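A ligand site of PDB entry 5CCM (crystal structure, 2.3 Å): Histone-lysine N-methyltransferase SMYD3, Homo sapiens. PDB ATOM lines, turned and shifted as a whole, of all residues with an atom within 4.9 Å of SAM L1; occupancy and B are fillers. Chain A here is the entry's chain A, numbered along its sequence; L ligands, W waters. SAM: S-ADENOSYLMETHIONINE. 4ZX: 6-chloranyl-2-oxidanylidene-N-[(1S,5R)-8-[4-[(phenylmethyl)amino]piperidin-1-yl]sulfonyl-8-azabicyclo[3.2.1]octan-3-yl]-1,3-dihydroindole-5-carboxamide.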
ATOM      1  N   ASN A  13     -19.625 -22.271 -42.025  1.00  0.00           N
ATOM      2  CA  ASN A  13     -20.911 -21.966 -41.374  1.00  0.00           C
ATOM      3  C   ASN A  13     -20.914 -21.659 -39.881  1.00  0.00           C
ATOM      4  O   ASN A  13     -21.956 -21.795 -39.224  1.00  0.00           O
ATOM      5  CB  ASN A  13     -21.908 -23.103 -41.662  1.00  0.00           C
ATOM      6  CG  ASN A  13     -21.422 -24.459 -41.166  1.00  0.00           C
ATOM      7  OD1 ASN A  13     -20.967 -24.612 -40.043  1.00  0.00           O
ATOM      8  ND2 ASN A  13     -21.553 -25.455 -42.015  1.00  0.00           N
ATOM      9  N   ARG A  14     -19.760 -21.251 -39.335  1.00  0.00           N
ATOM     10  CA  ARG A  14     -19.676 -20.898 -37.914  1.00  0.00           C
ATOM     11  C   ARG A  14     -18.703 -19.747 -37.677  1.00  0.00           C
ATOM     12  O   ARG A  14     -17.906 -19.755 -36.734  1.00  0.00           O
ATOM     13  CB  ARG A  14     -19.359 -22.118 -37.060  1.00  0.00           C
ATOM     14  CG  ARG A  14     -18.235 -23.006 -37.529  1.00  0.00           C
ATOM     15  CD  ARG A  14     -18.615 -24.450 -37.251  1.00  0.00           C
ATOM     16  NE  ARG A  14     -17.478 -25.308 -36.929  1.00  0.00           N
ATOM     17  CZ  ARG A  14     -17.574 -26.579 -36.552  1.00  0.00           C
ATOM     18  NH1 ARG A  14     -16.474 -27.273 -36.276  1.00  0.00           N
ATOM     19  NH2 ARG A  14     -18.761 -27.172 -36.423  1.00  0.00           N
ATOM     20  N   GLY A  15     -18.817 -18.735 -38.539  1.00  0.00           N
ATOM     21  CA  GLY A  15     -18.046 -17.525 -38.417  1.00  0.00           C
ATOM     22  C   GLY A  15     -16.567 -17.781 -38.609  1.00  0.00           C
ATOM     23  O   GLY A  15     -16.182 -18.721 -39.309  1.00  0.00           O
ATOM     24  N   ASN A  16     -15.746 -16.959 -37.972  1.00  0.00           N
ATOM     25  CA  ASN A  16     -14.321 -17.187 -38.019  1.00  0.00           C
ATOM     26  C   ASN A  16     -13.904 -18.326 -37.098  1.00  0.00           C
ATOM     27  O   ASN A  16     -14.675 -18.748 -36.223  1.00  0.00           O
ATOM     28  CB  ASN A  16     -13.540 -15.897 -37.717  1.00  0.00           C
ATOM     29  CG  ASN A  16     -13.961 -14.746 -38.619  1.00  0.00           C
ATOM     30  OD1 ASN A  16     -14.033 -13.609 -38.177  1.00  0.00           O
ATOM     31  ND2 ASN A  16     -14.276 -15.049 -39.872  1.00  0.00           N
ATOM     32  N   TYR A 124      -6.904 -11.733 -32.972  1.00  0.00           N
ATOM     33  CA  TYR A 124      -8.314 -11.365 -32.961  1.00  0.00           C
ATOM     34  C   TYR A 124      -8.452 -10.341 -31.837  1.00  0.00           C
ATOM     35  O   TYR A 124      -7.927 -10.567 -30.742  1.00  0.00           O
ATOM     36  CB  TYR A 124      -9.148 -12.615 -32.654  1.00  0.00           C
ATOM     37  CG  TYR A 124     -10.513 -12.718 -33.309  1.00  0.00           C
ATOM     38  CD1 TYR A 124     -10.685 -12.445 -34.659  1.00  0.00           C
ATOM     39  CD2 TYR A 124     -11.626 -13.147 -32.574  1.00  0.00           C
ATOM     40  CE1 TYR A 124     -11.923 -12.562 -35.256  1.00  0.00           C
ATOM     41  CE2 TYR A 124     -12.874 -13.274 -33.173  1.00  0.00           C
ATOM     42  CZ  TYR A 124     -13.012 -12.985 -34.519  1.00  0.00           C
ATOM     43  OH  TYR A 124     -14.227 -13.101 -35.138  1.00  0.00           O
ATOM     44  N   ASP A 128     -13.205  -7.433 -32.996  1.00  0.00           N
ATOM     45  CA  ASP A 128     -13.611  -8.483 -33.925  1.00  0.00           C
ATOM     46  C   ASP A 128     -14.602  -9.497 -33.342  1.00  0.00           C
ATOM     47  O   ASP A 128     -15.235 -10.224 -34.097  1.00  0.00           O
ATOM     48  CB  ASP A 128     -12.393  -9.236 -34.441  1.00  0.00           C
ATOM     49  CG  ASP A 128     -11.354  -8.322 -35.063  1.00  0.00           C
ATOM     50  OD1 ASP A 128     -11.717  -7.446 -35.867  1.00  0.00           O
ATOM     51  OD2 ASP A 128     -10.161  -8.485 -34.735  1.00  0.00           O
ATOM     52  N   LEU A 129     -14.731  -9.549 -32.015  1.00  0.00           N
ATOM     53  CA  LEU A 129     -15.500 -10.605 -31.356  1.00  0.00           C
ATOM     54  C   LEU A 129     -16.940 -10.730 -31.848  1.00  0.00           C
ATOM     55  O   LEU A 129     -17.589  -9.736 -32.158  1.00  0.00           O
ATOM     56  CB  LEU A 129     -15.496 -10.440 -29.834  1.00  0.00           C
ATOM     57  CG  LEU A 129     -14.147 -10.589 -29.147  1.00  0.00           C
ATOM     58  CD1 LEU A 129     -14.290 -10.347 -27.640  1.00  0.00           C
ATOM     59  CD2 LEU A 129     -13.523 -11.952 -29.401  1.00  0.00           C
ATOM     60  N   GLU A 130     -17.403 -11.960 -31.939  1.00  0.00           N
ATOM     61  CA  GLU A 130     -18.789 -12.233 -32.289  1.00  0.00           C
ATOM     62  C   GLU A 130     -19.709 -11.669 -31.221  1.00  0.00           C
ATOM     63  O   GLU A 130     -19.480 -11.872 -30.016  1.00  0.00           O
ATOM     64  CB  GLU A 130     -19.003 -13.745 -32.396  1.00  0.00           C
ATOM     65  CG  GLU A 130     -20.418 -14.162 -32.793  1.00  0.00           C
ATOM     66  CD  GLU A 130     -20.781 -13.702 -34.189  1.00  0.00           C
ATOM     67  OE1 GLU A 130     -20.235 -14.266 -35.149  1.00  0.00           O
ATOM     68  OE2 GLU A 130     -21.612 -12.772 -34.312  1.00  0.00           O
ATOM     69  N   ASN A 132     -23.328 -11.985 -31.890  1.00  0.00           N
ATOM     70  CA  ASN A 132     -24.594 -12.690 -32.169  1.00  0.00           C
ATOM     71  C   ASN A 132     -25.835 -11.803 -32.068  1.00  0.00           C
ATOM     72  O   ASN A 132     -26.910 -12.254 -31.661  1.00  0.00           O
ATOM     73  CB  ASN A 132     -24.784 -13.913 -31.244  1.00  0.00           C
ATOM     74  CG  ASN A 132     -23.788 -15.027 -31.530  1.00  0.00           C
ATOM     75  OD1 ASN A 132     -23.045 -15.443 -30.645  1.00  0.00           O
ATOM     76  ND2 ASN A 132     -23.775 -15.528 -32.761  1.00  0.00           N
ATOM     77  N   CYS A 180     -20.807 -14.055 -24.677  1.00  0.00           N
ATOM     78  CA  CYS A 180     -20.367 -15.235 -25.403  1.00  0.00           C
ATOM     79  C   CYS A 180     -18.859 -15.273 -25.684  1.00  0.00           C
ATOM     80  O   CYS A 180     -18.410 -16.088 -26.487  1.00  0.00           O
ATOM     81  CB  CYS A 180     -21.166 -15.376 -26.690  1.00  0.00           C
ATOM     82  SG  CYS A 180     -20.675 -14.235 -27.988  1.00  0.00           S
ATOM     83  N   ASN A 181     -18.066 -14.417 -25.033  1.00  0.00           N
ATOM     84  CA  ASN A 181     -16.599 -14.515 -25.137  1.00  0.00           C
ATOM     85  C   ASN A 181     -15.864 -14.450 -23.798  1.00  0.00           C
ATOM     86  O   ASN A 181     -14.635 -14.327 -23.766  1.00  0.00           O
ATOM     87  CB  ASN A 181     -16.050 -13.461 -26.093  1.00  0.00           C
ATOM     88  CG  ASN A 181     -16.562 -13.633 -27.509  1.00  0.00           C
ATOM     89  OD1 ASN A 181     -16.155 -14.543 -28.215  1.00  0.00           O
ATOM     90  ND2 ASN A 181     -17.483 -12.764 -27.912  1.00  0.00           N
ATOM     91  N   SER A 202     -10.735 -16.633 -28.191  1.00  0.00           N
ATOM     92  CA  SER A 202     -12.132 -16.644 -28.609  1.00  0.00           C
ATOM     93  C   SER A 202     -12.364 -16.981 -30.083  1.00  0.00           C
ATOM     94  O   SER A 202     -13.522 -17.057 -30.508  1.00  0.00           O
ATOM     95  CB  SER A 202     -12.802 -15.311 -28.267  1.00  0.00           C
ATOM     96  OG  SER A 202     -12.896 -15.140 -26.860  1.00  0.00           O
ATOM     97  N   LEU A 203     -11.296 -17.150 -30.869  1.00  0.00           N
ATOM     98  CA  LEU A 203     -11.401 -17.639 -32.244  1.00  0.00           C
ATOM     99  C   LEU A 203     -11.816 -19.101 -32.308  1.00  0.00           C
ATOM    100  O   LEU A 203     -12.461 -19.523 -33.249  1.00  0.00           O
ATOM    101  CB  LEU A 203     -10.071 -17.500 -33.008  1.00  0.00           C
ATOM    102  CG  LEU A 203      -9.877 -16.287 -33.893  1.00  0.00           C
ATOM    103  CD1 LEU A 203      -8.445 -16.213 -34.392  1.00  0.00           C
ATOM    104  CD2 LEU A 203     -10.832 -16.291 -35.079  1.00  0.00           C
ATOM    105  N   LEU A 204     -11.402 -19.879 -31.327  1.00  0.00           N
ATOM    106  CA  LEU A 204     -11.663 -21.315 -31.368  1.00  0.00           C
ATOM    107  C   LEU A 204     -13.167 -21.582 -31.252  1.00  0.00           C
ATOM    108  O   LEU A 204     -13.837 -21.053 -30.372  1.00  0.00           O
ATOM    109  CB  LEU A 204     -10.880 -22.037 -30.273  1.00  0.00           C
ATOM    110  CG  LEU A 204      -9.379 -22.134 -30.580  1.00  0.00           C
ATOM    111  CD1 LEU A 204      -8.577 -21.145 -29.760  1.00  0.00           C
ATOM    112  CD2 LEU A 204      -8.839 -23.524 -30.312  1.00  0.00           C
ATOM    113  N   ASN A 205     -13.687 -22.368 -32.195  1.00  0.00           N
ATOM    114  CA  ASN A 205     -15.076 -22.792 -32.179  1.00  0.00           C
ATOM    115  C   ASN A 205     -15.242 -24.006 -31.268  1.00  0.00           C
ATOM    116  O   ASN A 205     -14.259 -24.544 -30.758  1.00  0.00           O
ATOM    117  CB  ASN A 205     -15.565 -23.045 -33.603  1.00  0.00           C
ATOM    118  CG  ASN A 205     -15.866 -21.758 -34.354  1.00  0.00           C
ATOM    119  OD1 ASN A 205     -16.662 -20.959 -33.903  1.00  0.00           O
ATOM    120  ND2 ASN A 205     -15.219 -21.550 -35.489  1.00  0.00           N
ATOM    121  N   HIS A 206     -16.484 -24.411 -31.044  1.00  0.00           N
ATOM    122  CA  HIS A 206     -16.817 -25.390 -30.015  1.00  0.00           C
ATOM    123  C   HIS A 206     -16.962 -26.782 -30.576  1.00  0.00           C
ATOM    124  O   HIS A 206     -17.489 -26.956 -31.661  1.00  0.00           O
ATOM    125  CB  HIS A 206     -18.146 -25.023 -29.359  1.00  0.00           C
ATOM    126  CG  HIS A 206     -18.770 -26.163 -28.632  1.00  0.00           C
ATOM    127  ND1 HIS A 206     -18.442 -26.481 -27.332  1.00  0.00           N
ATOM    128  CD2 HIS A 206     -19.662 -27.096 -29.030  1.00  0.00           C
ATOM    129  CE1 HIS A 206     -19.134 -27.545 -26.949  1.00  0.00           C
ATOM    130  NE2 HIS A 206     -19.880 -27.937 -27.955  1.00  0.00           N
ATOM    131  N   TYR A 239     -16.461 -25.670 -24.970  1.00  0.00           N
ATOM    132  CA  TYR A 239     -16.934 -24.558 -24.179  1.00  0.00           C
ATOM    133  C   TYR A 239     -17.526 -24.986 -22.841  1.00  0.00           C
ATOM    134  O   TYR A 239     -17.586 -24.155 -21.917  1.00  0.00           O
ATOM    135  CB  TYR A 239     -17.997 -23.758 -24.947  1.00  0.00           C
ATOM    136  CG  TYR A 239     -17.539 -23.021 -26.209  1.00  0.00           C
ATOM    137  CD1 TYR A 239     -16.204 -23.034 -26.636  1.00  0.00           C
ATOM    138  CD2 TYR A 239     -18.437 -22.288 -26.947  1.00  0.00           C
ATOM    139  CE1 TYR A 239     -15.806 -22.351 -27.767  1.00  0.00           C
ATOM    140  CE2 TYR A 239     -18.053 -21.602 -28.079  1.00  0.00           C
ATOM    141  CZ  TYR A 239     -16.736 -21.630 -28.485  1.00  0.00           C
ATOM    142  OH  TYR A 239     -16.362 -20.953 -29.618  1.00  0.00           O
ATOM    143  N   TYR A 257     -24.479 -18.897 -26.490  1.00  0.00           N
ATOM    144  CA  TYR A 257     -23.640 -18.827 -27.690  1.00  0.00           C
ATOM    145  C   TYR A 257     -24.424 -18.799 -28.997  1.00  0.00           C
ATOM    146  O   TYR A 257     -23.826 -18.666 -30.057  1.00  0.00           O
ATOM    147  CB  TYR A 257     -22.674 -20.008 -27.707  1.00  0.00           C
ATOM    148  CG  TYR A 257     -21.684 -19.988 -26.576  1.00  0.00           C
ATOM    149  CD1 TYR A 257     -20.575 -19.152 -26.632  1.00  0.00           C
ATOM    150  CD2 TYR A 257     -21.842 -20.789 -25.441  1.00  0.00           C
ATOM    151  CE1 TYR A 257     -19.652 -19.119 -25.602  1.00  0.00           C
ATOM    152  CE2 TYR A 257     -20.926 -20.751 -24.398  1.00  0.00           C
ATOM    153  CZ  TYR A 257     -19.823 -19.913 -24.484  1.00  0.00           C
ATOM    154  OH  TYR A 257     -18.885 -19.850 -23.490  1.00  0.00           O
ATOM    155  N   CYS A 258     -25.751 -18.953 -28.928  1.00  0.00           N
ATOM    156  CA  CYS A 258     -26.604 -18.760 -30.096  1.00  0.00           C
ATOM    157  C   CYS A 258     -26.289 -19.667 -31.284  1.00  0.00           C
ATOM    158  O   CYS A 258     -26.314 -19.236 -32.427  1.00  0.00           O
ATOM    159  CB  CYS A 258     -26.586 -17.289 -30.546  1.00  0.00           C
ATOM    160  SG  CYS A 258     -27.489 -16.200 -29.431  1.00  0.00           S
ATOM    161  N   PHE A 259     -25.995 -20.936 -31.009  1.00  0.00           N
ATOM    162  CA  PHE A 259     -25.856 -21.896 -32.096  1.00  0.00           C
ATOM    163  C   PHE A 259     -26.329 -23.265 -31.669  1.00  0.00           C
ATOM    164  O   PHE A 259     -26.450 -23.551 -30.481  1.00  0.00           O
ATOM    165  CB  PHE A 259     -24.408 -21.962 -32.628  1.00  0.00           C
ATOM    166  CG  PHE A 259     -23.454 -22.691 -31.718  1.00  0.00           C
ATOM    167  CD1 PHE A 259     -22.822 -22.031 -30.685  1.00  0.00           C
ATOM    168  CD2 PHE A 259     -23.177 -24.033 -31.906  1.00  0.00           C
ATOM    169  CE1 PHE A 259     -21.922 -22.691 -29.862  1.00  0.00           C
ATOM    170  CE2 PHE A 259     -22.301 -24.701 -31.068  1.00  0.00           C
ATOM    171  CZ  PHE A 259     -21.664 -24.023 -30.056  1.00  0.00           C
ATOM    172  N   GLU A 260     -26.585 -24.079 -32.677  1.00  0.00           N
ATOM    173  CA  GLU A 260     -27.087 -25.441 -32.530  1.00  0.00           C
ATOM    174  C   GLU A 260     -25.933 -26.371 -32.874  1.00  0.00           C
ATOM    175  O   GLU A 260     -25.413 -26.313 -33.981  1.00  0.00           O
ATOM    176  CB  GLU A 260     -28.267 -25.672 -33.493  1.00  0.00           C
ATOM    177  CG  GLU A 260     -29.232 -24.501 -33.600  1.00  0.00           C
ATOM    178  CD  GLU A 260     -30.102 -24.316 -32.365  1.00  0.00           C
ATOM    179  OE1 GLU A 260     -30.168 -25.237 -31.525  1.00  0.00           O
ATOM    180  OE2 GLU A 260     -30.738 -23.238 -32.250  1.00  0.00           O
ATOM    181  N   CYS A 261     -25.537 -27.222 -31.943  1.00  0.00           N
ATOM    182  CA  CYS A 261     -24.381 -28.081 -32.185  1.00  0.00           C
ATOM    183  C   CYS A 261     -24.725 -29.280 -33.075  1.00  0.00           C
ATOM    184  O   CYS A 261     -25.621 -30.064 -32.745  1.00  0.00           O
ATOM    185  CB  CYS A 261     -23.830 -28.582 -30.865  1.00  0.00           C
ATOM    186  SG  CYS A 261     -22.222 -29.333 -31.129  1.00  0.00           S
HETATM  187  N   SAM L   1     -17.101 -18.161 -34.502  1.00  0.00           N
HETATM  188  CA  SAM L   1     -16.656 -17.104 -33.606  1.00  0.00           C
HETATM  189  C   SAM L   1     -16.242 -15.879 -34.368  1.00  0.00           C
HETATM  190  O   SAM L   1     -15.656 -14.950 -33.771  1.00  0.00           O
HETATM  191  OXT SAM L   1     -16.513 -15.811 -35.596  1.00  0.00           O
HETATM  192  CB  SAM L   1     -15.500 -17.622 -32.746  1.00  0.00           C
HETATM  193  CG  SAM L   1     -15.982 -18.488 -31.577  1.00  0.00           C
HETATM  194  SD  SAM L   1     -16.818 -17.589 -30.441  1.00  0.00           S
HETATM  195  CE  SAM L   1     -16.042 -17.666 -28.977  1.00  0.00           C
HETATM  196  C5' SAM L   1     -18.362 -18.228 -30.202  1.00  0.00           C
HETATM  197  C4' SAM L   1     -19.322 -18.166 -31.398  1.00  0.00           C
HETATM  198  O4' SAM L   1     -18.894 -18.889 -32.558  1.00  0.00           O
HETATM  199  C3' SAM L   1     -20.689 -18.760 -31.046  1.00  0.00           C
HETATM  200  O3' SAM L   1     -21.539 -17.815 -30.382  1.00  0.00           O
HETATM  201  C2' SAM L   1     -21.221 -19.173 -32.393  1.00  0.00           C
HETATM  202  O2' SAM L   1     -21.737 -18.035 -33.080  1.00  0.00           O
HETATM  203  C1' SAM L   1     -19.973 -19.660 -33.109  1.00  0.00           C
HETATM  204  N9  SAM L   1     -19.698 -21.090 -32.895  1.00  0.00           N
HETATM  205  C8  SAM L   1     -18.791 -21.611 -32.043  1.00  0.00           C
HETATM  206  N7  SAM L   1     -18.769 -22.966 -32.095  1.00  0.00           N
HETATM  207  C5  SAM L   1     -19.698 -23.324 -33.002  1.00  0.00           C
HETATM  208  C6  SAM L   1     -20.206 -24.597 -33.567  1.00  0.00           C
HETATM  209  N6  SAM L   1     -19.715 -25.802 -33.157  1.00  0.00           N
HETATM  210  N1  SAM L   1     -21.177 -24.529 -34.500  1.00  0.00           N
HETATM  211  C2  SAM L   1     -21.674 -23.352 -34.937  1.00  0.00           C
HETATM  212  N3  SAM L   1     -21.260 -22.169 -34.475  1.00  0.00           N
HETATM  213  C4  SAM L   1     -20.302 -22.088 -33.519  1.00  0.00           C
HETATM  214 CL1  4ZX L   2     -13.953 -23.469 -22.599  1.00  0.00          CL
HETATM  215  C02 4ZX L   2     -14.497 -21.843 -22.880  1.00  0.00           C
HETATM  216  C03 4ZX L   2     -14.247 -21.348 -24.158  1.00  0.00           C
HETATM  217  C05 4ZX L   2     -14.632 -20.067 -24.454  1.00  0.00           C
HETATM  218  C06 4ZX L   2     -15.274 -19.253 -23.527  1.00  0.00           C
HETATM  219  C07 4ZX L   2     -15.554 -17.935 -24.168  1.00  0.00           C
HETATM  220  C10 4ZX L   2     -14.981 -18.120 -25.564  1.00  0.00           C
HETATM  221  O11 4ZX L   2     -14.969 -17.299 -26.448  1.00  0.00           O
HETATM  222  N12 4ZX L   2     -14.472 -19.400 -25.640  1.00  0.00           N
HETATM  223  C14 4ZX L   2     -15.544 -19.715 -22.263  1.00  0.00           C
HETATM  224  C16 4ZX L   2     -15.169 -21.034 -21.926  1.00  0.00           C
HETATM  225  C17 4ZX L   2     -15.444 -21.445 -20.522  1.00  0.00           C
HETATM  226  O18 4ZX L   2     -15.297 -20.611 -19.639  1.00  0.00           O
HETATM  227  N19 4ZX L   2     -15.770 -22.701 -20.132  1.00  0.00           N
HETATM  228  C21 4ZX L   2     -16.009 -23.145 -18.748  1.00  0.00           C
HETATM  229  C23 4ZX L   2     -14.685 -23.218 -17.943  1.00  0.00           C
HETATM  230  C26 4ZX L   2     -14.008 -24.604 -17.906  1.00  0.00           C
HETATM  231  C28 4ZX L   2     -13.552 -25.098 -19.270  1.00  0.00           C
HETATM  232  C31 4ZX L   2     -14.819 -25.694 -19.885  1.00  0.00           C
HETATM  233  C34 4ZX L   2     -15.887 -25.692 -18.776  1.00  0.00           C
HETATM  234  C36 4ZX L   2     -16.804 -24.464 -18.734  1.00  0.00           C
HETATM  235  N39 4ZX L   2     -15.086 -25.550 -17.564  1.00  0.00           N
HETATM  236  S40 4ZX L   2     -14.767 -26.895 -16.639  1.00  0.00           S
HETATM  237  O41 4ZX L   2     -16.062 -27.534 -16.434  1.00  0.00           O
HETATM  238  O42 4ZX L   2     -13.643 -27.493 -17.340  1.00  0.00           O
HETATM  239  N43 4ZX L   2     -14.319 -26.206 -15.193  1.00  0.00           N
HETATM  240  C44 4ZX L   2     -15.308 -25.347 -14.506  1.00  0.00           C
HETATM  241  C47 4ZX L   2     -16.203 -26.218 -13.627  1.00  0.00           C
HETATM  242  C50 4ZX L   2     -15.338 -27.063 -12.688  1.00  0.00           C
HETATM  243  C52 4ZX L   2     -14.201 -27.834 -13.386  1.00  0.00           C
HETATM  244  C55 4ZX L   2     -13.392 -26.960 -14.321  1.00  0.00           C
HETATM  245  N58 4ZX L   2     -16.171 -27.897 -11.848  1.00  0.00           N
HETATM  246  C60 4ZX L   2     -17.002 -28.978 -12.372  1.00  0.00           C
HETATM  247  C63 4ZX L   2     -17.941 -29.383 -11.264  1.00  0.00           C
HETATM  248  C64 4ZX L   2     -17.588 -30.432 -10.394  1.00  0.00           C
HETATM  249  C66 4ZX L   2     -18.454 -30.787  -9.358  1.00  0.00           C
HETATM  250  C68 4ZX L   2     -19.662 -30.105  -9.182  1.00  0.00           C
HETATM  251  C70 4ZX L   2     -20.016 -29.059 -10.034  1.00  0.00           C
HETATM  252  C72 4ZX L   2     -19.154 -28.690 -11.069  1.00  0.00           C
HETATM  253  O   HOH W   1     -17.846 -13.544 -36.353  1.00  0.00           O
HETATM  254  O   HOH W   2     -22.890 -26.716 -35.226  1.00  0.00           O
HETATM  255  O   HOH W   3     -24.337 -18.354 -33.592  1.00  0.00           O
HETATM  256  O   HOH W   4     -19.677 -17.002 -34.956  1.00  0.00           O
HETATM  257  O   HOH W   5     -20.567 -28.460 -33.767  1.00  0.00           O
HETATM  258  O   HOH W   6     -15.563 -13.906 -31.176  1.00  0.00           O
HETATM  259  O   HOH W   7     -23.069 -20.167 -35.673  1.00  0.00           O
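OD1 of Asn 181 lies close to O11 of 4ZX L2.
An oxygen (O3') of SAM L1 lies within hydrogen-bond range of the backbone carbonyl oxygen (O) of Tyr 257.
The side-chain hydroxyl (OH) of Tyr 124 lies within hydrogen-bond range of an oxygen (O) of SAM L1, 2.7 Å away.
An oxygen (OXT) of SAM L1 sits at hydrogen-bond distance from the backbone NH (N) of Asn 16, at 2.7 Å.
N of SAM L1 sits at hydrogen-bond distance from O of Arg 14 (2.9 Å).
The side-chain amide oxygen (OD1) of Asn 205 sits at hydrogen-bond distance from a nitrogen (N) of SAM L1, at 2.9 Å.
The side-chain amide oxygen (OD1) of Asn 132 sits at hydrogen-bond distance from an oxygen (O3') of SAM L1 (2.8 Å).
The backbone NH (N) of His 206 lies within hydrogen-bond range of a nitrogen (N7) of SAM L1.
The backbone carbonyl oxygen (O) of Asn 16 is in hydrogen-bond range of a nitrogen (N) of SAM L1 (3.0 Å).
The backbone carbonyl oxygen (O) of His 206 sits at hydrogen-bond distance from a nitrogen (N6) of SAM L1 (2.9 Å).
The side-chain hydroxyl (OG) of Ser 202 sits at hydrogen-bond distance from an oxygen (O11) of 4ZX L2 (3.0 Å).
The backbone carbonyl oxygen (O) of Tyr 239 is in hydrogen-bond range of a nitrogen (N19) of 4ZX L2 (2.9 Å).
The side-chain hydroxyl (OH) of Tyr 124 is in hydrogen-bond range of the side-chain amide oxygen (OD1) of Asn 16, at 3.1 Å.
OD1 of Asn 205 sits close to O of Arg 14, 3.3 Å away.
OH of Tyr 124 lies within hydrogen-bond range of O of Asp 128 (3.2 Å).
ND1 of His 206 sits at hydrogen-bond distance from N of Tyr 239 (3.2 Å).
ND2 of Asn 205 lies within hydrogen-bond range of O of Asn 16.
The backbone carbonyl oxygen (O) of Glu 130 sits at hydrogen-bond distance from the side-chain amide nitrogen (ND2) of Asn 181, at 3.0 Å.
The backbone carbonyl oxygen (O) of Leu 204 lies within hydrogen-bond range of the side-chain hydroxyl (OH) of Tyr 239 (2.6 Å).
The side-chain amide oxygen of Asn 132 sits at hydrogen-bond distance from the side-chain sulfur of Cys 180 (3.8 Å).
O of Ser 202 sits close to SD of SAM L1 (3.3 Å).
OH of Tyr 239 sits close to SD of SAM L1 (3.5 Å).
Merely in contact with SAM L1: Gly 15, Glu 130, Cys 180, Asn 181, Leu 203, Leu 204 and Phe 259.
Hydrophobic or aromatic side chains within 4 Å of SAM L1: Tyr 124, His 206, Tyr 239, Tyr 257 and Phe 259.
Of the 22 residues printed, 16 come within 4 Å of SAM L1.
The nearest printed residue that does not touch SAM L1 is Asn 13 (4.6 Å).
Water W3 lies within hydrogen-bond range of O of Cys 258 (2.5 Å), O2' of SAM L1 (2.7 Å) and ND2 of Asn 132 (3.0 Å).
Water W1 bridges an oxygen (OXT) of SAM L1 and the side-chain carboxylate (OE1) of Glu 130.
Water W6 lies within hydrogen-bond range of N of Glu 130 (2.8 Å), O of SAM L1 (2.8 Å) and OD1 of Asn 181 (3.1 Å).
Water W5 bridges N6 of SAM L1 (2.9 Å) and NH2 of Arg 14 (3.5 Å).
Water W4 bridges OE1 of Glu 130 (2.8 Å) and N of SAM L1 (2.9 Å).
Water W2 lies within hydrogen-bond range of the backbone carbonyl oxygen of Glu 260 (2.8 Å) and a nitrogen (N1) of SAM L1 (2.9 Å).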
